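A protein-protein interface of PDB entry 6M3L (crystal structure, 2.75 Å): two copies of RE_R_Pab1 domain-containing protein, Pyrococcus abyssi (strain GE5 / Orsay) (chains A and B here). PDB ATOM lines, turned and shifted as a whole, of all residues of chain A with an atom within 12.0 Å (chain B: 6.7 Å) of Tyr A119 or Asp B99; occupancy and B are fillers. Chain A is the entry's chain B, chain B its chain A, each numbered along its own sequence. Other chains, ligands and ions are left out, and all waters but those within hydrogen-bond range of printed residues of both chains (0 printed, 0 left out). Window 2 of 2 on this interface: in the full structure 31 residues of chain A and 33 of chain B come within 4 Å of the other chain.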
ATOM      1  N   THR A 114     -12.762   4.800  29.615  1.00  0.00           N
ATOM      2  CA  THR A 114     -12.320   6.078  30.143  1.00  0.00           C
ATOM      3  C   THR A 114     -13.375   7.119  29.800  1.00  0.00           C
ATOM      4  O   THR A 114     -14.121   6.979  28.826  1.00  0.00           O
ATOM      5  CB  THR A 114     -10.955   6.496  29.582  1.00  0.00           C
ATOM      6  OG1 THR A 114     -11.127   7.089  28.290  1.00  0.00           O
ATOM      7  CG2 THR A 114     -10.036   5.293  29.462  1.00  0.00           C
ATOM      8  N   ASN A 115     -13.442   8.164  30.620  1.00  0.00           N
ATOM      9  CA  ASN A 115     -14.443   9.211  30.460  1.00  0.00           C
ATOM     10  C   ASN A 115     -14.048  10.245  29.415  1.00  0.00           C
ATOM     11  O   ASN A 115     -14.381  11.427  29.561  1.00  0.00           O
ATOM     12  CB  ASN A 115     -14.713   9.882  31.808  1.00  0.00           C
ATOM     13  CG  ASN A 115     -15.236   8.908  32.844  1.00  0.00           C
ATOM     14  OD1 ASN A 115     -15.821   7.882  32.502  1.00  0.00           O
ATOM     15  ND2 ASN A 115     -15.024   9.222  34.120  1.00  0.00           N
ATOM     16  N   GLU A 116     -13.355   9.833  28.359  1.00  0.00           N
ATOM     17  CA  GLU A 116     -12.871  10.758  27.347  1.00  0.00           C
ATOM     18  C   GLU A 116     -13.659  10.616  26.051  1.00  0.00           C
ATOM     19  O   GLU A 116     -14.165   9.541  25.715  1.00  0.00           O
ATOM     20  CB  GLU A 116     -11.381  10.541  27.076  1.00  0.00           C
ATOM     21  CG  GLU A 116     -10.484  10.925  28.240  1.00  0.00           C
ATOM     22  CD  GLU A 116      -9.047  11.145  27.815  1.00  0.00           C
ATOM     23  OE1 GLU A 116      -8.680  10.704  26.706  1.00  0.00           O
ATOM     24  OE2 GLU A 116      -8.286  11.766  28.585  1.00  0.00           O
ATOM     25  N   GLU A 117     -13.758  11.726  25.327  1.00  0.00           N
ATOM     26  CA  GLU A 117     -14.437  11.790  24.042  1.00  0.00           C
ATOM     27  C   GLU A 117     -13.510  12.477  23.053  1.00  0.00           C
ATOM     28  O   GLU A 117     -13.000  13.566  23.332  1.00  0.00           O
ATOM     29  CB  GLU A 117     -15.763  12.549  24.155  1.00  0.00           C
ATOM     30  CG  GLU A 117     -16.436  12.841  22.824  1.00  0.00           C
ATOM     31  CD  GLU A 117     -17.427  13.987  22.916  1.00  0.00           C
ATOM     32  OE1 GLU A 117     -17.402  14.711  23.933  1.00  0.00           O
ATOM     33  OE2 GLU A 117     -18.227  14.166  21.974  1.00  0.00           O
ATOM     34  N   LEU A 118     -13.284  11.836  21.911  1.00  0.00           N
ATOM     35  CA  LEU A 118     -12.387  12.355  20.884  1.00  0.00           C
ATOM     36  C   LEU A 118     -13.246  12.751  19.688  1.00  0.00           C
ATOM     37  O   LEU A 118     -13.376  12.011  18.713  1.00  0.00           O
ATOM     38  CB  LEU A 118     -11.333  11.322  20.522  1.00  0.00           C
ATOM     39  CG  LEU A 118     -10.157  11.816  19.682  1.00  0.00           C
ATOM     40  CD1 LEU A 118      -9.604  13.109  20.252  1.00  0.00           C
ATOM     41  CD2 LEU A 118      -9.078  10.754  19.633  1.00  0.00           C
ATOM     42  N   TYR A 119     -13.842  13.939  19.779  1.00  0.00           N
ATOM     43  CA  TYR A 119     -14.781  14.453  18.782  1.00  0.00           C
ATOM     44  C   TYR A 119     -15.873  13.420  18.488  1.00  0.00           C
ATOM     45  O   TYR A 119     -15.963  12.841  17.408  1.00  0.00           O
ATOM     46  CB  TYR A 119     -14.045  14.875  17.507  1.00  0.00           C
ATOM     47  CG  TYR A 119     -12.970  15.906  17.751  1.00  0.00           C
ATOM     48  CD1 TYR A 119     -13.288  17.252  17.893  1.00  0.00           C
ATOM     49  CD2 TYR A 119     -11.636  15.534  17.849  1.00  0.00           C
ATOM     50  CE1 TYR A 119     -12.301  18.201  18.122  1.00  0.00           C
ATOM     51  CE2 TYR A 119     -10.644  16.474  18.077  1.00  0.00           C
ATOM     52  CZ  TYR A 119     -10.982  17.804  18.212  1.00  0.00           C
ATOM     53  OH  TYR A 119      -9.996  18.738  18.438  1.00  0.00           O
ATOM     54  N   GLY A 120     -16.698  13.198  19.507  1.00  0.00           N
ATOM     55  CA  GLY A 120     -17.818  12.292  19.410  1.00  0.00           C
ATOM     56  C   GLY A 120     -17.484  10.820  19.475  1.00  0.00           C
ATOM     57  O   GLY A 120     -18.405   9.995  19.430  1.00  0.00           O
ATOM     58  N   PHE A 121     -16.210  10.454  19.575  1.00  0.00           N
ATOM     59  CA  PHE A 121     -15.806   9.057  19.672  1.00  0.00           C
ATOM     60  C   PHE A 121     -15.372   8.749  21.099  1.00  0.00           C
ATOM     61  O   PHE A 121     -14.529   9.454  21.662  1.00  0.00           O
ATOM     62  CB  PHE A 121     -14.675   8.735  18.693  1.00  0.00           C
ATOM     63  CG  PHE A 121     -15.130   8.557  17.272  1.00  0.00           C
ATOM     64  CD1 PHE A 121     -15.552   9.645  16.524  1.00  0.00           C
ATOM     65  CD2 PHE A 121     -15.130   7.302  16.681  1.00  0.00           C
ATOM     66  CE1 PHE A 121     -15.967   9.487  15.217  1.00  0.00           C
ATOM     67  CE2 PHE A 121     -15.548   7.138  15.368  1.00  0.00           C
ATOM     68  CZ  PHE A 121     -15.965   8.232  14.639  1.00  0.00           C
ATOM     69  N   ASN A 122     -15.945   7.696  21.677  1.00  0.00           N
ATOM     70  CA  ASN A 122     -15.593   7.300  23.033  1.00  0.00           C
ATOM     71  C   ASN A 122     -14.247   6.587  23.042  1.00  0.00           C
ATOM     72  O   ASN A 122     -13.990   5.710  22.210  1.00  0.00           O
ATOM     73  CB  ASN A 122     -16.678   6.398  23.623  1.00  0.00           C
ATOM     74  CG  ASN A 122     -17.921   7.167  24.031  1.00  0.00           C
ATOM     75  OD1 ASN A 122     -17.849   8.343  24.390  1.00  0.00           O
ATOM     76  ND2 ASN A 122     -19.073   6.503  23.984  1.00  0.00           N
ATOM     77  N   ILE A 123     -13.385   6.968  23.984  1.00  0.00           N
ATOM     78  CA  ILE A 123     -12.039   6.418  24.092  1.00  0.00           C
ATOM     79  C   ILE A 123     -12.033   5.322  25.145  1.00  0.00           C
ATOM     80  O   ILE A 123     -12.670   5.450  26.198  1.00  0.00           O
ATOM     81  CB  ILE A 123     -11.015   7.519  24.428  1.00  0.00           C
ATOM     82  CG1 ILE A 123     -11.027   8.611  23.356  1.00  0.00           C
ATOM     83  CG2 ILE A 123      -9.620   6.929  24.561  1.00  0.00           C
ATOM     84  CD1 ILE A 123     -10.319   8.223  22.069  1.00  0.00           C
ATOM     85  N   TYR A 124     -11.328   4.230  24.852  1.00  0.00           N
ATOM     86  CA  TYR A 124     -11.158   3.117  25.773  1.00  0.00           C
ATOM     87  C   TYR A 124      -9.686   2.717  25.808  1.00  0.00           C
ATOM     88  O   TYR A 124      -8.860   3.221  25.041  1.00  0.00           O
ATOM     89  CB  TYR A 124     -12.023   1.910  25.375  1.00  0.00           C
ATOM     90  CG  TYR A 124     -13.508   2.175  25.329  1.00  0.00           C
ATOM     91  CD1 TYR A 124     -14.350   1.679  26.315  1.00  0.00           C
ATOM     92  CD2 TYR A 124     -14.073   2.911  24.295  1.00  0.00           C
ATOM     93  CE1 TYR A 124     -15.714   1.911  26.275  1.00  0.00           C
ATOM     94  CE2 TYR A 124     -15.436   3.153  24.250  1.00  0.00           C
ATOM     95  CZ  TYR A 124     -16.249   2.650  25.242  1.00  0.00           C
ATOM     96  OH  TYR A 124     -17.602   2.886  25.197  1.00  0.00           O
ATOM     97  N   LEU B  94     -14.656  19.041   5.619  1.00  0.00           N
ATOM     98  CA  LEU B  94     -13.363  19.709   5.565  1.00  0.00           C
ATOM     99  C   LEU B  94     -13.263  20.781   6.641  1.00  0.00           C
ATOM    100  O   LEU B  94     -12.177  21.024   7.181  1.00  0.00           O
ATOM    101  CB  LEU B  94     -13.148  20.319   4.182  1.00  0.00           C
ATOM    102  CG  LEU B  94     -12.516  19.369   3.163  1.00  0.00           C
ATOM    103  CD1 LEU B  94     -12.632  19.932   1.750  1.00  0.00           C
ATOM    104  CD2 LEU B  94     -11.080  19.015   3.512  1.00  0.00           C
ATOM    105  N   LYS B  95     -14.387  21.426   6.965  1.00  0.00           N
ATOM    106  CA  LYS B  95     -14.420  22.378   8.068  1.00  0.00           C
ATOM    107  C   LYS B  95     -14.331  21.660   9.408  1.00  0.00           C
ATOM    108  O   LYS B  95     -13.840  22.228  10.389  1.00  0.00           O
ATOM    109  CB  LYS B  95     -15.685  23.230   7.996  1.00  0.00           C
ATOM    110  CG  LYS B  95     -15.579  24.332   6.965  1.00  0.00           C
ATOM    111  CD  LYS B  95     -14.406  25.248   7.249  1.00  0.00           C
ATOM    112  CE  LYS B  95     -13.983  25.972   5.983  1.00  0.00           C
ATOM    113  NZ  LYS B  95     -13.299  25.042   5.037  1.00  0.00           N
ATOM    114  N   PHE B  96     -14.796  20.412   9.460  1.00  0.00           N
ATOM    115  CA  PHE B  96     -14.587  19.585  10.641  1.00  0.00           C
ATOM    116  C   PHE B  96     -13.120  19.212  10.767  1.00  0.00           C
ATOM    117  O   PHE B  96     -12.568  19.196  11.873  1.00  0.00           O
ATOM    118  CB  PHE B  96     -15.455  18.331  10.577  1.00  0.00           C
ATOM    119  CG  PHE B  96     -15.129  17.316  11.637  1.00  0.00           C
ATOM    120  CD1 PHE B  96     -15.598  17.473  12.931  1.00  0.00           C
ATOM    121  CD2 PHE B  96     -14.353  16.207  11.342  1.00  0.00           C
ATOM    122  CE1 PHE B  96     -15.303  16.541  13.903  1.00  0.00           C
ATOM    123  CE2 PHE B  96     -14.055  15.275  12.311  1.00  0.00           C
ATOM    124  CZ  PHE B  96     -14.534  15.441  13.593  1.00  0.00           C
ATOM    125  N   ALA B  97     -12.480  18.893   9.642  1.00  0.00           N
ATOM    126  CA  ALA B  97     -11.064  18.557   9.666  1.00  0.00           C
ATOM    127  C   ALA B  97     -10.226  19.769  10.054  1.00  0.00           C
ATOM    128  O   ALA B  97      -9.246  19.638  10.788  1.00  0.00           O
ATOM    129  CB  ALA B  97     -10.629  18.016   8.307  1.00  0.00           C
ATOM    130  N   ASP B  98     -10.641  20.966   9.662  1.00  0.00           N
ATOM    131  CA  ASP B  98      -9.867  22.139  10.045  1.00  0.00           C
ATOM    132  C   ASP B  98      -9.932  22.357  11.550  1.00  0.00           C
ATOM    133  O   ASP B  98      -9.003  22.921  12.137  1.00  0.00           O
ATOM    134  CB  ASP B  98     -10.373  23.371   9.297  1.00  0.00           C
ATOM    135  CG  ASP B  98      -9.690  23.563   7.956  1.00  0.00           C
ATOM    136  OD1 ASP B  98      -8.441  23.564   7.924  1.00  0.00           O
ATOM    137  OD2 ASP B  98     -10.397  23.715   6.936  1.00  0.00           O
ATOM    138  N   ASP B  99     -11.011  21.903  12.186  1.00  0.00           N
ATOM    139  CA  ASP B  99     -11.199  22.037  13.622  1.00  0.00           C
ATOM    140  C   ASP B  99     -10.580  20.904  14.439  1.00  0.00           C
ATOM    141  O   ASP B  99     -10.286  21.107  15.622  1.00  0.00           O
ATOM    142  CB  ASP B  99     -12.695  22.110  13.926  1.00  0.00           C
ATOM    143  CG  ASP B  99     -13.349  23.338  13.326  1.00  0.00           C
ATOM    144  OD1 ASP B  99     -12.669  24.063  12.571  1.00  0.00           O
ATOM    145  OD2 ASP B  99     -14.544  23.573  13.601  1.00  0.00           O
ATOM    146  N   VAL B 100     -10.366  19.724  13.849  1.00  0.00           N
ATOM    147  CA  VAL B 100      -9.768  18.612  14.587  1.00  0.00           C
ATOM    148  C   VAL B 100      -8.286  18.882  14.801  1.00  0.00           C
ATOM    149  O   VAL B 100      -7.540  19.138  13.847  1.00  0.00           O
ATOM    150  CB  VAL B 100      -9.991  17.285  13.847  1.00  0.00           C
ATOM    151  CG1 VAL B 100      -9.015  16.225  14.346  1.00  0.00           C
ATOM    152  CG2 VAL B 100     -11.413  16.817  14.023  1.00  0.00           C
ATOM    153  N   LYS B 101      -7.846  18.834  16.063  1.00  0.00           N
ATOM    154  CA  LYS B 101      -6.441  19.055  16.358  1.00  0.00           C
ATOM    155  C   LYS B 101      -5.786  18.028  17.287  1.00  0.00           C
ATOM    156  O   LYS B 101      -4.555  18.035  17.402  1.00  0.00           O
ATOM    157  CB  LYS B 101      -6.283  20.457  16.967  1.00  0.00           C
ATOM    158  CG  LYS B 101      -4.898  21.000  16.931  1.00  0.00           C
ATOM    159  CD  LYS B 101      -4.205  20.645  15.643  1.00  0.00           C
ATOM    160  CE  LYS B 101      -2.782  21.095  15.729  1.00  0.00           C
ATOM    161  NZ  LYS B 101      -2.256  20.730  17.070  1.00  0.00           N
ATOM    162  N   SER B 102      -6.546  17.149  17.932  1.00  0.00           N
ATOM    163  CA  SER B 102      -6.014  16.017  18.685  1.00  0.00           C
ATOM    164  C   SER B 102      -6.454  14.704  18.046  1.00  0.00           C
ATOM    165  O   SER B 102      -7.548  14.612  17.487  1.00  0.00           O
ATOM    166  CB  SER B 102      -6.429  16.068  20.162  1.00  0.00           C
ATOM    167  OG  SER B 102      -7.830  16.184  20.313  1.00  0.00           O
ATOM    168  N   TYR B 103      -5.597  13.683  18.115  1.00  0.00           N
ATOM    169  CA  TYR B 103      -5.828  12.456  17.365  1.00  0.00           C
ATOM    170  C   TYR B 103      -5.699  11.247  18.288  1.00  0.00           C
ATOM    171  O   TYR B 103      -5.137  11.332  19.382  1.00  0.00           O
ATOM    172  CB  TYR B 103      -4.839  12.349  16.192  1.00  0.00           C
ATOM    173  CG  TYR B 103      -4.829  13.582  15.306  1.00  0.00           C
ATOM    174  CD1 TYR B 103      -5.661  13.678  14.200  1.00  0.00           C
ATOM    175  CD2 TYR B 103      -3.985  14.651  15.582  1.00  0.00           C
ATOM    176  CE1 TYR B 103      -5.655  14.805  13.395  1.00  0.00           C
ATOM    177  CE2 TYR B 103      -3.973  15.781  14.784  1.00  0.00           C
ATOM    178  CZ  TYR B 103      -4.809  15.854  13.691  1.00  0.00           C
ATOM    179  OH  TYR B 103      -4.797  16.979  12.896  1.00  0.00           O
ATOM    180  N   LYS B 133     -17.787   3.982  18.352  1.00  0.00           N
ATOM    181  CA  LYS B 133     -18.958   4.832  18.197  1.00  0.00           C
ATOM    182  C   LYS B 133     -20.118   4.027  17.642  1.00  0.00           C
ATOM    183  O   LYS B 133     -19.980   3.358  16.614  1.00  0.00           O
ATOM    184  CB  LYS B 133     -18.662   6.030  17.290  1.00  0.00           C
ATOM    185  CG  LYS B 133     -19.835   6.986  17.161  1.00  0.00           C
ATOM    186  CD  LYS B 133     -19.503   8.170  16.273  1.00  0.00           C
ATOM    187  CE  LYS B 133     -20.466   9.323  16.524  1.00  0.00           C
ATOM    188  NZ  LYS B 133     -20.035  10.566  15.824  1.00  0.00           N
ATOM    189  N   GLU B 193     -19.320   9.313   8.860  1.00  0.00           N
ATOM    190  CA  GLU B 193     -18.695   8.945  10.121  1.00  0.00           C
ATOM    191  C   GLU B 193     -17.399   8.178   9.894  1.00  0.00           C
ATOM    192  O   GLU B 193     -16.466   8.282  10.697  1.00  0.00           O
ATOM    193  CB  GLU B 193     -19.669   8.100  10.947  1.00  0.00           C
ATOM    194  CG  GLU B 193     -20.939   8.821  11.438  1.00  0.00           C
ATOM    195  CD  GLU B 193     -20.735   9.880  12.507  1.00  0.00           C
ATOM    196  OE1 GLU B 193     -19.710  10.590  12.489  1.00  0.00           O
ATOM    197  OE2 GLU B 193     -21.633  10.015  13.370  1.00  0.00           O
ATOM    198  N   LYS B 196     -14.930  10.768   9.139  1.00  0.00           N
ATOM    199  CA  LYS B 196     -14.596  11.378  10.422  1.00  0.00           C
ATOM    200  C   LYS B 196     -13.615  10.515  11.206  1.00  0.00           C
ATOM    201  O   LYS B 196     -12.657  11.033  11.791  1.00  0.00           O
ATOM    202  CB  LYS B 196     -15.859  11.630  11.250  1.00  0.00           C
ATOM    203  CG  LYS B 196     -16.745  12.754  10.744  1.00  0.00           C
ATOM    204  CD  LYS B 196     -17.363  13.507  11.915  1.00  0.00           C
ATOM    205  CE  LYS B 196     -18.856  13.711  11.730  1.00  0.00           C
ATOM    206  NZ  LYS B 196     -19.183  15.115  11.359  1.00  0.00           N
ATOM    207  N   ILE B 200      -9.897  11.881  12.595  1.00  0.00           N
ATOM    208  CA  ILE B 200      -9.426  11.926  13.979  1.00  0.00           C
ATOM    209  C   ILE B 200      -8.475  10.791  14.335  1.00  0.00           C
ATOM    210  O   ILE B 200      -7.894  10.807  15.431  1.00  0.00           O
ATOM    211  CB  ILE B 200     -10.597  11.935  14.981  1.00  0.00           C
ATOM    212  CG1 ILE B 200     -11.266  10.566  15.047  1.00  0.00           C
ATOM    213  CG2 ILE B 200     -11.594  13.030  14.619  1.00  0.00           C
ATOM    214  CD1 ILE B 200     -12.182  10.408  16.228  1.00  0.00           C
ATOM    215  N   LYS B 206      -5.712  12.068   8.436  1.00  0.00           N
ATOM    216  CA  LYS B 206      -6.488  13.275   8.197  1.00  0.00           C
ATOM    217  C   LYS B 206      -6.077  13.965   6.909  1.00  0.00           C
ATOM    218  O   LYS B 206      -6.927  14.371   6.109  1.00  0.00           O
ATOM    219  CB  LYS B 206      -6.296  14.225   9.363  1.00  0.00           C
ATOM    220  CG  LYS B 206      -7.124  15.441   9.286  1.00  0.00           C
ATOM    221  CD  LYS B 206      -6.842  16.202  10.520  1.00  0.00           C
ATOM    222  CE  LYS B 206      -7.800  17.294  10.657  1.00  0.00           C
ATOM    223  NZ  LYS B 206      -7.596  18.000  11.939  1.00  0.00           N
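The backbone NH of Lys B101 lies within hydrogen-bond range of the side-chain hydroxyl of Tyr A119 (3.2 Å).
OE2 of Glu A117 is in hydrogen-bond range of N of Gly A120, 3.1 Å away.
OH of Tyr B103 sits at hydrogen-bond distance from NZ of Lys B206 (3.1 Å).
The side-chain amino group (NZ) of Lys B133 is in salt-bridge range of the side-chain carboxylate (OE2) of Glu B193, 3.0 Å away.
Ser B102 touches Leu A118.
Tyr B103 touches Leu A118 (C to CD2, 3.7 Å).
CZ of Phe B96 touches CB of Tyr A119 (3.98 Å).
Tyr A119 touches Asp B99 (OH to O, 3.7 Å).
Tyr A119 touches Val B100 (OH to CA, 3.9 Å).
Tyr A119 touches Ser B102 (CE2 to OG, 3.6 Å).
Lys B133 touches Gly A120 (CE to O, 3.6 Å).
Phe A121 touches Lys B133.
O of Glu B193 touches CZ of Phe A121, 3.97 Å away.
Ile B200 touches Phe A121 (CD1 to CD1, 3.5 Å).
Of the printed residues of chain B, Leu A118 touches Ser B102, Tyr B103 and Ile B200.
Printed residues of chain B within 4 Å of Tyr A119: Phe B96 (3.98 Å), Asp B99 (3.7 Å), Val B100 (3.9 Å), Lys B101 (3.2 Å) and Ser B102 (3.6 Å).
Of the printed residues of chain B, Gly A120 touches Lys B133.
Of the printed residues of chain B, Phe A121 touches Lys B133 (3.8 Å), Glu B193 (3.97 Å) and Ile B200 (3.5 Å).
Tyr A124 touches none of the printed residues of chain B.
No residue of chain A comes within 4 Å of Lys B95.
Of the printed residues of chain A, Phe B96 touches Tyr A119 (3.98 Å).
Ala B97 touches none of the printed residues of chain A.
Asp B98 touches none of the printed residues of chain A.
Val B100 touches one residue of chain A.
Printed residues of chain A within 4 Å of Lys B101: Tyr A119 (3.2 Å).
Tyr B103 touches just one residue of chain A: Leu A118.
Ile B200 touches just these residues of chain A: Leu A118 and Phe A121.
The nearest printed residue of chain B that does not touch Tyr A119 is Ile B200 (4.1 Å).
Of the 15 printed residues of chain B, 9 touch a printed residue of chain A.
Along chain B the printed residues that touch a printed residue of chain A span positions 96 to 200.
Printed residues of chain A that touch a printed residue of chain B: Leu A118, Tyr A119, Gly A120 and Phe A121.
Hydrophobic or aromatic side chains of chain A that line the printed part of chain B: Leu A118, Tyr A119 and Phe A121.
Among the printed residues, 12 pairs touch across the chains.
Among the printed residues, no Asp or Glu carboxylate lies within 4 Å of a Lys or Arg side-chain nitrogen of the other chain.
No position is printed for both chains.
Of the 12 pairs that touch across the chains among the printed residues, none has its exchanged pair printed and touching as well.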
